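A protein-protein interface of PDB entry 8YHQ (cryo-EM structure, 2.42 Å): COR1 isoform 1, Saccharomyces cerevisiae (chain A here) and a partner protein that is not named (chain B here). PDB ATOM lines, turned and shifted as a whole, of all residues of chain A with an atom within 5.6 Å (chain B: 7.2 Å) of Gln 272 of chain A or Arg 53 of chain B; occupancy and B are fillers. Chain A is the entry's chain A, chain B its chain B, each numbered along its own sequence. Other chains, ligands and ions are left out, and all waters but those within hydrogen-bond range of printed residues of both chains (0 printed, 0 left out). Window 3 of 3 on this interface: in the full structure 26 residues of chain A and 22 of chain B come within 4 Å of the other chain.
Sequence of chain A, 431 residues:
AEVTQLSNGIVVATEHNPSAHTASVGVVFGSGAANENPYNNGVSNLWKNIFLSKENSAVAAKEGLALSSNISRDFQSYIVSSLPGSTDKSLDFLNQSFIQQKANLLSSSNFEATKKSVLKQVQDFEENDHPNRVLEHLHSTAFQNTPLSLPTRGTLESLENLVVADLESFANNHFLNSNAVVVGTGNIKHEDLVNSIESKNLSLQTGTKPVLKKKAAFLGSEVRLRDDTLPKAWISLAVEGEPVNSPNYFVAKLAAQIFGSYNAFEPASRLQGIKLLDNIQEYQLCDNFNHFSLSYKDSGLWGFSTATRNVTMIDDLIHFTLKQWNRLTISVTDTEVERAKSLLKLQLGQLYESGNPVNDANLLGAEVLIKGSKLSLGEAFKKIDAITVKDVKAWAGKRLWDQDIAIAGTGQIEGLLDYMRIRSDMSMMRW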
ATOM      1  N   SER A 261      17.958  -6.216   3.157  1.00  0.00           N
ATOM      2  CA  SER A 261      18.611  -7.389   3.720  1.00  0.00           C
ATOM      3  C   SER A 261      19.509  -8.023   2.667  1.00  0.00           C
ATOM      4  O   SER A 261      19.315  -7.838   1.464  1.00  0.00           O
ATOM      5  CB  SER A 261      17.587  -8.404   4.233  1.00  0.00           C
ATOM      6  OG  SER A 261      16.806  -8.916   3.178  1.00  0.00           O
ATOM      7  N   TYR A 262      20.494  -8.786   3.139  1.00  0.00           N
ATOM      8  CA  TYR A 262      21.577  -9.270   2.295  1.00  0.00           C
ATOM      9  C   TYR A 262      22.034 -10.653   2.734  1.00  0.00           C
ATOM     10  O   TYR A 262      22.131 -10.934   3.930  1.00  0.00           O
ATOM     11  CB  TYR A 262      22.754  -8.297   2.348  1.00  0.00           C
ATOM     12  CG  TYR A 262      23.963  -8.672   1.544  1.00  0.00           C
ATOM     13  CD1 TYR A 262      23.892  -8.825   0.176  1.00  0.00           C
ATOM     14  CD2 TYR A 262      25.190  -8.841   2.155  1.00  0.00           C
ATOM     15  CE1 TYR A 262      24.992  -9.149  -0.552  1.00  0.00           C
ATOM     16  CE2 TYR A 262      26.296  -9.165   1.434  1.00  0.00           C
ATOM     17  CZ  TYR A 262      26.195  -9.317   0.080  1.00  0.00           C
ATOM     18  OH  TYR A 262      27.304  -9.641  -0.647  1.00  0.00           O
ATOM     19  N   ALA A 268      21.533 -13.897  -6.422  1.00  0.00           N
ATOM     20  CA  ALA A 268      20.603 -12.828  -6.759  1.00  0.00           C
ATOM     21  C   ALA A 268      20.535 -11.745  -5.695  1.00  0.00           C
ATOM     22  O   ALA A 268      20.179 -10.606  -6.012  1.00  0.00           O
ATOM     23  CB  ALA A 268      19.208 -13.392  -6.996  1.00  0.00           C
ATOM     24  N   SER A 269      20.857 -12.070  -4.448  1.00  0.00           N
ATOM     25  CA  SER A 269      20.892 -11.073  -3.393  1.00  0.00           C
ATOM     26  C   SER A 269      22.067 -10.116  -3.526  1.00  0.00           C
ATOM     27  O   SER A 269      22.031  -9.038  -2.929  1.00  0.00           O
ATOM     28  CB  SER A 269      20.929 -11.771  -2.038  1.00  0.00           C
ATOM     29  OG  SER A 269      20.857 -10.855  -0.972  1.00  0.00           O
ATOM     30  N   ARG A 270      23.092 -10.471  -4.298  1.00  0.00           N
ATOM     31  CA  ARG A 270      24.226  -9.594  -4.544  1.00  0.00           C
ATOM     32  C   ARG A 270      23.941  -8.536  -5.602  1.00  0.00           C
ATOM     33  O   ARG A 270      24.730  -7.597  -5.739  1.00  0.00           O
ATOM     34  CB  ARG A 270      25.448 -10.417  -4.969  1.00  0.00           C
ATOM     35  CG  ARG A 270      25.987 -11.363  -3.914  1.00  0.00           C
ATOM     36  CD  ARG A 270      27.414 -11.808  -4.194  1.00  0.00           C
ATOM     37  NE  ARG A 270      27.497 -12.716  -5.332  1.00  0.00           N
ATOM     38  CZ  ARG A 270      27.480 -14.048  -5.270  1.00  0.00           C
ATOM     39  NH1 ARG A 270      27.565 -14.749  -6.392  1.00  0.00           N
ATOM     40  NH2 ARG A 270      27.378 -14.696  -4.115  1.00  0.00           N
ATOM     41  N   LEU A 271      22.834  -8.656  -6.335  1.00  0.00           N
ATOM     42  CA  LEU A 271      22.498  -7.775  -7.442  1.00  0.00           C
ATOM     43  C   LEU A 271      21.424  -6.750  -7.098  1.00  0.00           C
ATOM     44  O   LEU A 271      20.934  -6.064  -7.996  1.00  0.00           O
ATOM     45  CB  LEU A 271      22.032  -8.599  -8.639  1.00  0.00           C
ATOM     46  CG  LEU A 271      22.926  -9.724  -9.147  1.00  0.00           C
ATOM     47  CD1 LEU A 271      22.178 -10.565 -10.137  1.00  0.00           C
ATOM     48  CD2 LEU A 271      24.177  -9.187  -9.770  1.00  0.00           C
ATOM     49  N   GLN A 272      21.046  -6.631  -5.829  1.00  0.00           N
ATOM     50  CA  GLN A 272      20.004  -5.698  -5.435  1.00  0.00           C
ATOM     51  C   GLN A 272      20.451  -4.253  -5.611  1.00  0.00           C
ATOM     52  O   GLN A 272      21.633  -3.922  -5.492  1.00  0.00           O
ATOM     53  CB  GLN A 272      19.605  -5.931  -3.984  1.00  0.00           C
ATOM     54  CG  GLN A 272      18.921  -7.238  -3.716  1.00  0.00           C
ATOM     55  CD  GLN A 272      18.507  -7.397  -2.277  1.00  0.00           C
ATOM     56  OE1 GLN A 272      17.342  -7.225  -1.932  1.00  0.00           O
ATOM     57  NE2 GLN A 272      19.458  -7.730  -1.428  1.00  0.00           N
ATOM     58  N   GLY A 273      19.481  -3.387  -5.889  1.00  0.00           N
ATOM     59  CA  GLY A 273      19.717  -1.967  -6.038  1.00  0.00           C
ATOM     60  C   GLY A 273      19.894  -1.231  -4.731  1.00  0.00           C
ATOM     61  O   GLY A 273      19.055  -0.413  -4.348  1.00  0.00           O
ATOM     62  N   ILE A 274      20.995  -1.518  -4.045  1.00  0.00           N
ATOM     63  CA  ILE A 274      21.314  -0.934  -2.750  1.00  0.00           C
ATOM     64  C   ILE A 274      22.752  -0.441  -2.818  1.00  0.00           C
ATOM     65  O   ILE A 274      23.670  -1.226  -3.073  1.00  0.00           O
ATOM     66  CB  ILE A 274      21.121  -1.945  -1.598  1.00  0.00           C
ATOM     67  CG1 ILE A 274      19.680  -2.466  -1.562  1.00  0.00           C
ATOM     68  CG2 ILE A 274      21.472  -1.319  -0.262  1.00  0.00           C
ATOM     69  CD1 ILE A 274      19.464  -3.688  -0.721  1.00  0.00           C
ATOM     70  N   LEU A 277      25.930  -1.907  -1.011  1.00  0.00           N
ATOM     71  CA  LEU A 277      26.571  -3.122  -1.493  1.00  0.00           C
ATOM     72  C   LEU A 277      27.774  -2.836  -2.374  1.00  0.00           C
ATOM     73  O   LEU A 277      28.653  -3.691  -2.498  1.00  0.00           O
ATOM     74  CB  LEU A 277      25.558  -3.977  -2.252  1.00  0.00           C
ATOM     75  CG  LEU A 277      24.341  -4.485  -1.477  1.00  0.00           C
ATOM     76  CD1 LEU A 277      23.513  -5.399  -2.346  1.00  0.00           C
ATOM     77  CD2 LEU A 277      24.730  -5.186  -0.201  1.00  0.00           C
ATOM     78  N   ARG A 339      11.315   2.334  -5.372  1.00  0.00           N
ATOM     79  CA  ARG A 339      11.654   0.928  -5.204  1.00  0.00           C
ATOM     80  C   ARG A 339      11.143   0.397  -3.871  1.00  0.00           C
ATOM     81  O   ARG A 339      10.537  -0.677  -3.811  1.00  0.00           O
ATOM     82  CB  ARG A 339      13.169   0.764  -5.316  1.00  0.00           C
ATOM     83  CG  ARG A 339      13.713  -0.645  -5.202  1.00  0.00           C
ATOM     84  CD  ARG A 339      15.207  -0.650  -5.000  1.00  0.00           C
ATOM     85  NE  ARG A 339      15.692  -1.958  -4.578  1.00  0.00           N
ATOM     86  CZ  ARG A 339      15.836  -2.367  -3.322  1.00  0.00           C
ATOM     87  NH1 ARG A 339      16.278  -3.584  -3.094  1.00  0.00           N
ATOM     88  NH2 ARG A 339      15.555  -1.591  -2.291  1.00  0.00           N
ATOM     89  N   ALA B  48      20.930 -10.757 -15.819  1.00  0.00           N
ATOM     90  CA  ALA B  48      20.425 -11.094 -14.497  1.00  0.00           C
ATOM     91  C   ALA B  48      20.308  -9.878 -13.594  1.00  0.00           C
ATOM     92  O   ALA B  48      19.525  -9.907 -12.641  1.00  0.00           O
ATOM     93  CB  ALA B  48      21.327 -12.132 -13.834  1.00  0.00           C
ATOM     94  N   LEU B  49      21.072  -8.822 -13.863  1.00  0.00           N
ATOM     95  CA  LEU B  49      20.987  -7.610 -13.065  1.00  0.00           C
ATOM     96  C   LEU B  49      19.724  -6.826 -13.393  1.00  0.00           C
ATOM     97  O   LEU B  49      19.026  -6.365 -12.489  1.00  0.00           O
ATOM     98  CB  LEU B  49      22.233  -6.758 -13.293  1.00  0.00           C
ATOM     99  CG  LEU B  49      22.372  -5.414 -12.578  1.00  0.00           C
ATOM    100  CD1 LEU B  49      22.499  -5.591 -11.104  1.00  0.00           C
ATOM    101  CD2 LEU B  49      23.564  -4.680 -13.096  1.00  0.00           C
ATOM    102  N   LYS B  50      19.409  -6.686 -14.678  1.00  0.00           N
ATOM    103  CA  LYS B  50      18.236  -5.924 -15.080  1.00  0.00           C
ATOM    104  C   LYS B  50      16.938  -6.584 -14.634  1.00  0.00           C
ATOM    105  O   LYS B  50      15.961  -5.885 -14.347  1.00  0.00           O
ATOM    106  CB  LYS B  50      18.237  -5.732 -16.590  1.00  0.00           C
ATOM    107  CG  LYS B  50      17.557  -4.474 -17.036  1.00  0.00           C
ATOM    108  CD  LYS B  50      17.035  -4.606 -18.437  1.00  0.00           C
ATOM    109  CE  LYS B  50      16.689  -3.254 -19.058  1.00  0.00           C
ATOM    110  NZ  LYS B  50      16.809  -3.275 -20.546  1.00  0.00           N
ATOM    111  N   LEU B  51      16.899  -7.915 -14.583  1.00  0.00           N
ATOM    112  CA  LEU B  51      15.708  -8.609 -14.106  1.00  0.00           C
ATOM    113  C   LEU B  51      15.439  -8.294 -12.639  1.00  0.00           C
ATOM    114  O   LEU B  51      14.291  -8.075 -12.240  1.00  0.00           O
ATOM    115  CB  LEU B  51      15.872 -10.110 -14.317  1.00  0.00           C
ATOM    116  CG  LEU B  51      14.685 -11.018 -13.995  1.00  0.00           C
ATOM    117  CD1 LEU B  51      13.633 -10.920 -15.065  1.00  0.00           C
ATOM    118  CD2 LEU B  51      15.154 -12.433 -13.835  1.00  0.00           C
ATOM    119  N   VAL B  52      16.487  -8.281 -11.820  1.00  0.00           N
ATOM    120  CA  VAL B  52      16.328  -7.981 -10.401  1.00  0.00           C
ATOM    121  C   VAL B  52      15.871  -6.540 -10.208  1.00  0.00           C
ATOM    122  O   VAL B  52      15.038  -6.247  -9.345  1.00  0.00           O
ATOM    123  CB  VAL B  52      17.638  -8.273  -9.645  1.00  0.00           C
ATOM    124  CG1 VAL B  52      17.639  -7.647  -8.270  1.00  0.00           C
ATOM    125  CG2 VAL B  52      17.858  -9.751  -9.533  1.00  0.00           C
ATOM    126  N   ARG B  53      16.407  -5.619 -11.010  1.00  0.00           N
ATOM    127  CA  ARG B  53      16.091  -4.207 -10.829  1.00  0.00           C
ATOM    128  C   ARG B  53      14.701  -3.873 -11.355  1.00  0.00           C
ATOM    129  O   ARG B  53      13.973  -3.089 -10.739  1.00  0.00           O
ATOM    130  CB  ARG B  53      17.143  -3.338 -11.515  1.00  0.00           C
ATOM    131  CG  ARG B  53      18.563  -3.518 -11.017  1.00  0.00           C
ATOM    132  CD  ARG B  53      18.761  -3.066  -9.611  1.00  0.00           C
ATOM    133  NE  ARG B  53      20.154  -3.178  -9.196  1.00  0.00           N
ATOM    134  CZ  ARG B  53      21.059  -2.203  -9.224  1.00  0.00           C
ATOM    135  NH1 ARG B  53      22.285  -2.453  -8.811  1.00  0.00           N
ATOM    136  NH2 ARG B  53      20.769  -0.986  -9.648  1.00  0.00           N
ATOM    137  N   GLU B  54      14.316  -4.449 -12.493  1.00  0.00           N
ATOM    138  CA  GLU B  54      13.002  -4.180 -13.064  1.00  0.00           C
ATOM    139  C   GLU B  54      11.887  -4.721 -12.181  1.00  0.00           C
ATOM    140  O   GLU B  54      10.882  -4.041 -11.950  1.00  0.00           O
ATOM    141  CB  GLU B  54      12.907  -4.785 -14.458  1.00  0.00           C
ATOM    142  CG  GLU B  54      13.598  -4.015 -15.528  1.00  0.00           C
ATOM    143  CD  GLU B  54      13.302  -4.568 -16.903  1.00  0.00           C
ATOM    144  OE1 GLU B  54      12.796  -5.706 -16.987  1.00  0.00           O
ATOM    145  OE2 GLU B  54      13.573  -3.868 -17.900  1.00  0.00           O
ATOM    146  N   SER B  55      12.031  -5.955 -11.699  1.00  0.00           N
ATOM    147  CA  SER B  55      10.973  -6.570 -10.907  1.00  0.00           C
ATOM    148  C   SER B  55      10.860  -5.947  -9.522  1.00  0.00           C
ATOM    149  O   SER B  55       9.775  -5.952  -8.935  1.00  0.00           O
ATOM    150  CB  SER B  55      11.213  -8.072 -10.800  1.00  0.00           C
ATOM    151  OG  SER B  55      12.387  -8.360 -10.068  1.00  0.00           O
ATOM    152  N   GLU B  56      11.957  -5.415  -8.983  1.00  0.00           N
ATOM    153  CA  GLU B  56      11.896  -4.733  -7.695  1.00  0.00           C
ATOM    154  C   GLU B  56      11.000  -3.507  -7.763  1.00  0.00           C
ATOM    155  O   GLU B  56      10.270  -3.210  -6.812  1.00  0.00           O
ATOM    156  CB  GLU B  56      13.295  -4.331  -7.239  1.00  0.00           C
ATOM    157  CG  GLU B  56      14.025  -5.384  -6.472  1.00  0.00           C
ATOM    158  CD  GLU B  56      15.415  -4.951  -6.050  1.00  0.00           C
ATOM    159  OE1 GLU B  56      16.038  -4.143  -6.768  1.00  0.00           O
ATOM    160  OE2 GLU B  56      15.886  -5.415  -4.995  1.00  0.00           O
ATOM    161  N   LEU B  57      11.050  -2.777  -8.876  1.00  0.00           N
ATOM    162  CA  LEU B  57      10.225  -1.588  -9.032  1.00  0.00           C
ATOM    163  C   LEU B  57       8.762  -1.938  -9.269  1.00  0.00           C
ATOM    164  O   LEU B  57       7.882  -1.124  -8.981  1.00  0.00           O
ATOM    165  CB  LEU B  57      10.759  -0.731 -10.177  1.00  0.00           C
ATOM    166  CG  LEU B  57      12.121  -0.070  -9.963  1.00  0.00           C
ATOM    167  CD1 LEU B  57      12.576   0.597 -11.224  1.00  0.00           C
ATOM    168  CD2 LEU B  57      12.089   0.928  -8.843  1.00  0.00           C
ATOM    169  N   LEU B  58       8.485  -3.127  -9.798  1.00  0.00           N
ATOM    170  CA  LEU B  58       7.125  -3.622  -9.938  1.00  0.00           C
ATOM    171  C   LEU B  58       6.623  -4.356  -8.702  1.00  0.00           C
ATOM    172  O   LEU B  58       5.418  -4.601  -8.600  1.00  0.00           O
ATOM    173  CB  LEU B  58       7.026  -4.564 -11.137  1.00  0.00           C
ATOM    174  CG  LEU B  58       7.162  -4.008 -12.545  1.00  0.00           C
ATOM    175  CD1 LEU B  58       7.064  -5.146 -13.511  1.00  0.00           C
ATOM    176  CD2 LEU B  58       6.114  -2.976 -12.851  1.00  0.00           C
ATOM    177  N   THR B  61       9.557 -10.957  -6.808  1.00  0.00           N
ATOM    178  CA  THR B  61      10.778 -11.716  -6.584  1.00  0.00           C
ATOM    179  C   THR B  61      10.676 -13.059  -7.298  1.00  0.00           C
ATOM    180  O   THR B  61       9.604 -13.470  -7.744  1.00  0.00           O
ATOM    181  CB  THR B  61      11.041 -11.918  -5.088  1.00  0.00           C
ATOM    182  OG1 THR B  61       9.826 -12.284  -4.427  1.00  0.00           O
ATOM    183  CG2 THR B  61      11.599 -10.648  -4.462  1.00  0.00           C
ATOM    184  N   TYR B  84       3.929  -9.821 -17.260  1.00  0.00           N
ATOM    185  CA  TYR B  84       5.373  -9.633 -17.176  1.00  0.00           C
ATOM    186  C   TYR B  84       6.061 -10.896 -16.674  1.00  0.00           C
ATOM    187  O   TYR B  84       7.112 -11.292 -17.191  1.00  0.00           O
ATOM    188  CB  TYR B  84       5.692  -8.444 -16.268  1.00  0.00           C
ATOM    189  CG  TYR B  84       7.157  -8.242 -15.952  1.00  0.00           C
ATOM    190  CD1 TYR B  84       7.963  -7.465 -16.763  1.00  0.00           C
ATOM    191  CD2 TYR B  84       7.729  -8.812 -14.827  1.00  0.00           C
ATOM    192  CE1 TYR B  84       9.291  -7.279 -16.469  1.00  0.00           C
ATOM    193  CE2 TYR B  84       9.048  -8.636 -14.534  1.00  0.00           C
ATOM    194  CZ  TYR B  84       9.828  -7.869 -15.352  1.00  0.00           C
ATOM    195  OH  TYR B  84      11.150  -7.698 -15.037  1.00  0.00           O
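O of Leu 271 of chain A sits at hydrogen-bond distance from NE of Arg 53 of chain B, 3.2 Å away.
The side-chain carboxylate of Glu 56 of chain B is in salt-bridge range of the guanidinium group of Arg 339 of chain A, 2.7 Å away.
The guanidinium group (NE) of Arg 53 of chain B lies close to the backbone NH (N) of Gly 273 of chain A (3.4 Å).
The side-chain amide nitrogen (NE2) of Gln 272 of chain A sits at hydrogen-bond distance from the backbone carbonyl oxygen (O) of Ser 261 of chain A (2.9 Å).
The backbone carbonyl oxygen (O) of Ser 269 of chain A lies within hydrogen-bond range of the side-chain amide nitrogen (NE2) of Gln 272 of chain A (3.3 Å).
OG of Ser 55 of chain B sits at hydrogen-bond distance from O of Val 52 of chain B, 3.5 Å away.
Among the printed residues, pairs that only touch across the chains: Leu 271 of chain A with Ala 48 of chain B (3.7 Å), Leu 271 of chain A with Leu 49 of chain B (3.5 Å), Leu 271 of chain A with Val 52 of chain B (3.7 Å), Gln 272 of chain A with Arg 53 of chain B (3.7 Å), Gln 272 of chain A with Glu 56 of chain B (3.8 Å), Gly 273 of chain A with Glu 56 of chain B (3.6 Å) and Arg 339 of chain A with Leu 57 of chain B (3.7 Å).
Of chain B, only Arg 53 (3.7 Å) and Glu 56 (3.8 Å) come within 4 Å of Gln 272 of chain A.
Of chain A, only Leu 271 (3.2 Å), Gln 272 (3.7 Å) and Gly 273 (3.4 Å) come within 4 Å of Arg 53 of chain B.
Of the printed residues of chain B, Gly 273 of chain A touches Arg 53 and Glu 56.
Of the printed residues of chain A, Glu 56 of chain B touches Gln 272 (3.8 Å), Gly 273 (3.6 Å) and Arg 339 (2.7 Å).
Printed residues of chain A within 4 Å of Val 52 of chain B: Leu 271 (3.7 Å).
Of the printed residues of chain A, Leu 49 of chain B touches Leu 271.
Ile 274 of chain A touches none of the printed residues of chain B.
The nearest residue of chain A that does not touch Arg 53 of chain B is Ile 274 of chain A (5.0 Å).
Of the 11 printed residues of chain A, 4 touch a printed residue of chain B.
Hydrophobic or aromatic side chains of chain A within 4 Å of the printed part of chain B: Leu 271.
Of the 13 printed residues of chain B, 6 touch a printed residue of chain A.
Printed residues of chain B that touch a printed residue of chain A: Ala 48, Leu 49, Val 52, Arg 53, Glu 56 and Leu 57.
Hydrophobic or aromatic side chains of chain B that line the printed part of chain A: Leu 49, Val 52 and Leu 57.
Among the printed residues, Asp or Glu carboxylates within 4 Å of a Lys or Arg side-chain nitrogen of the other chain: Arg 339 of chain A with Glu 56 of chain B (2.7 Å).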
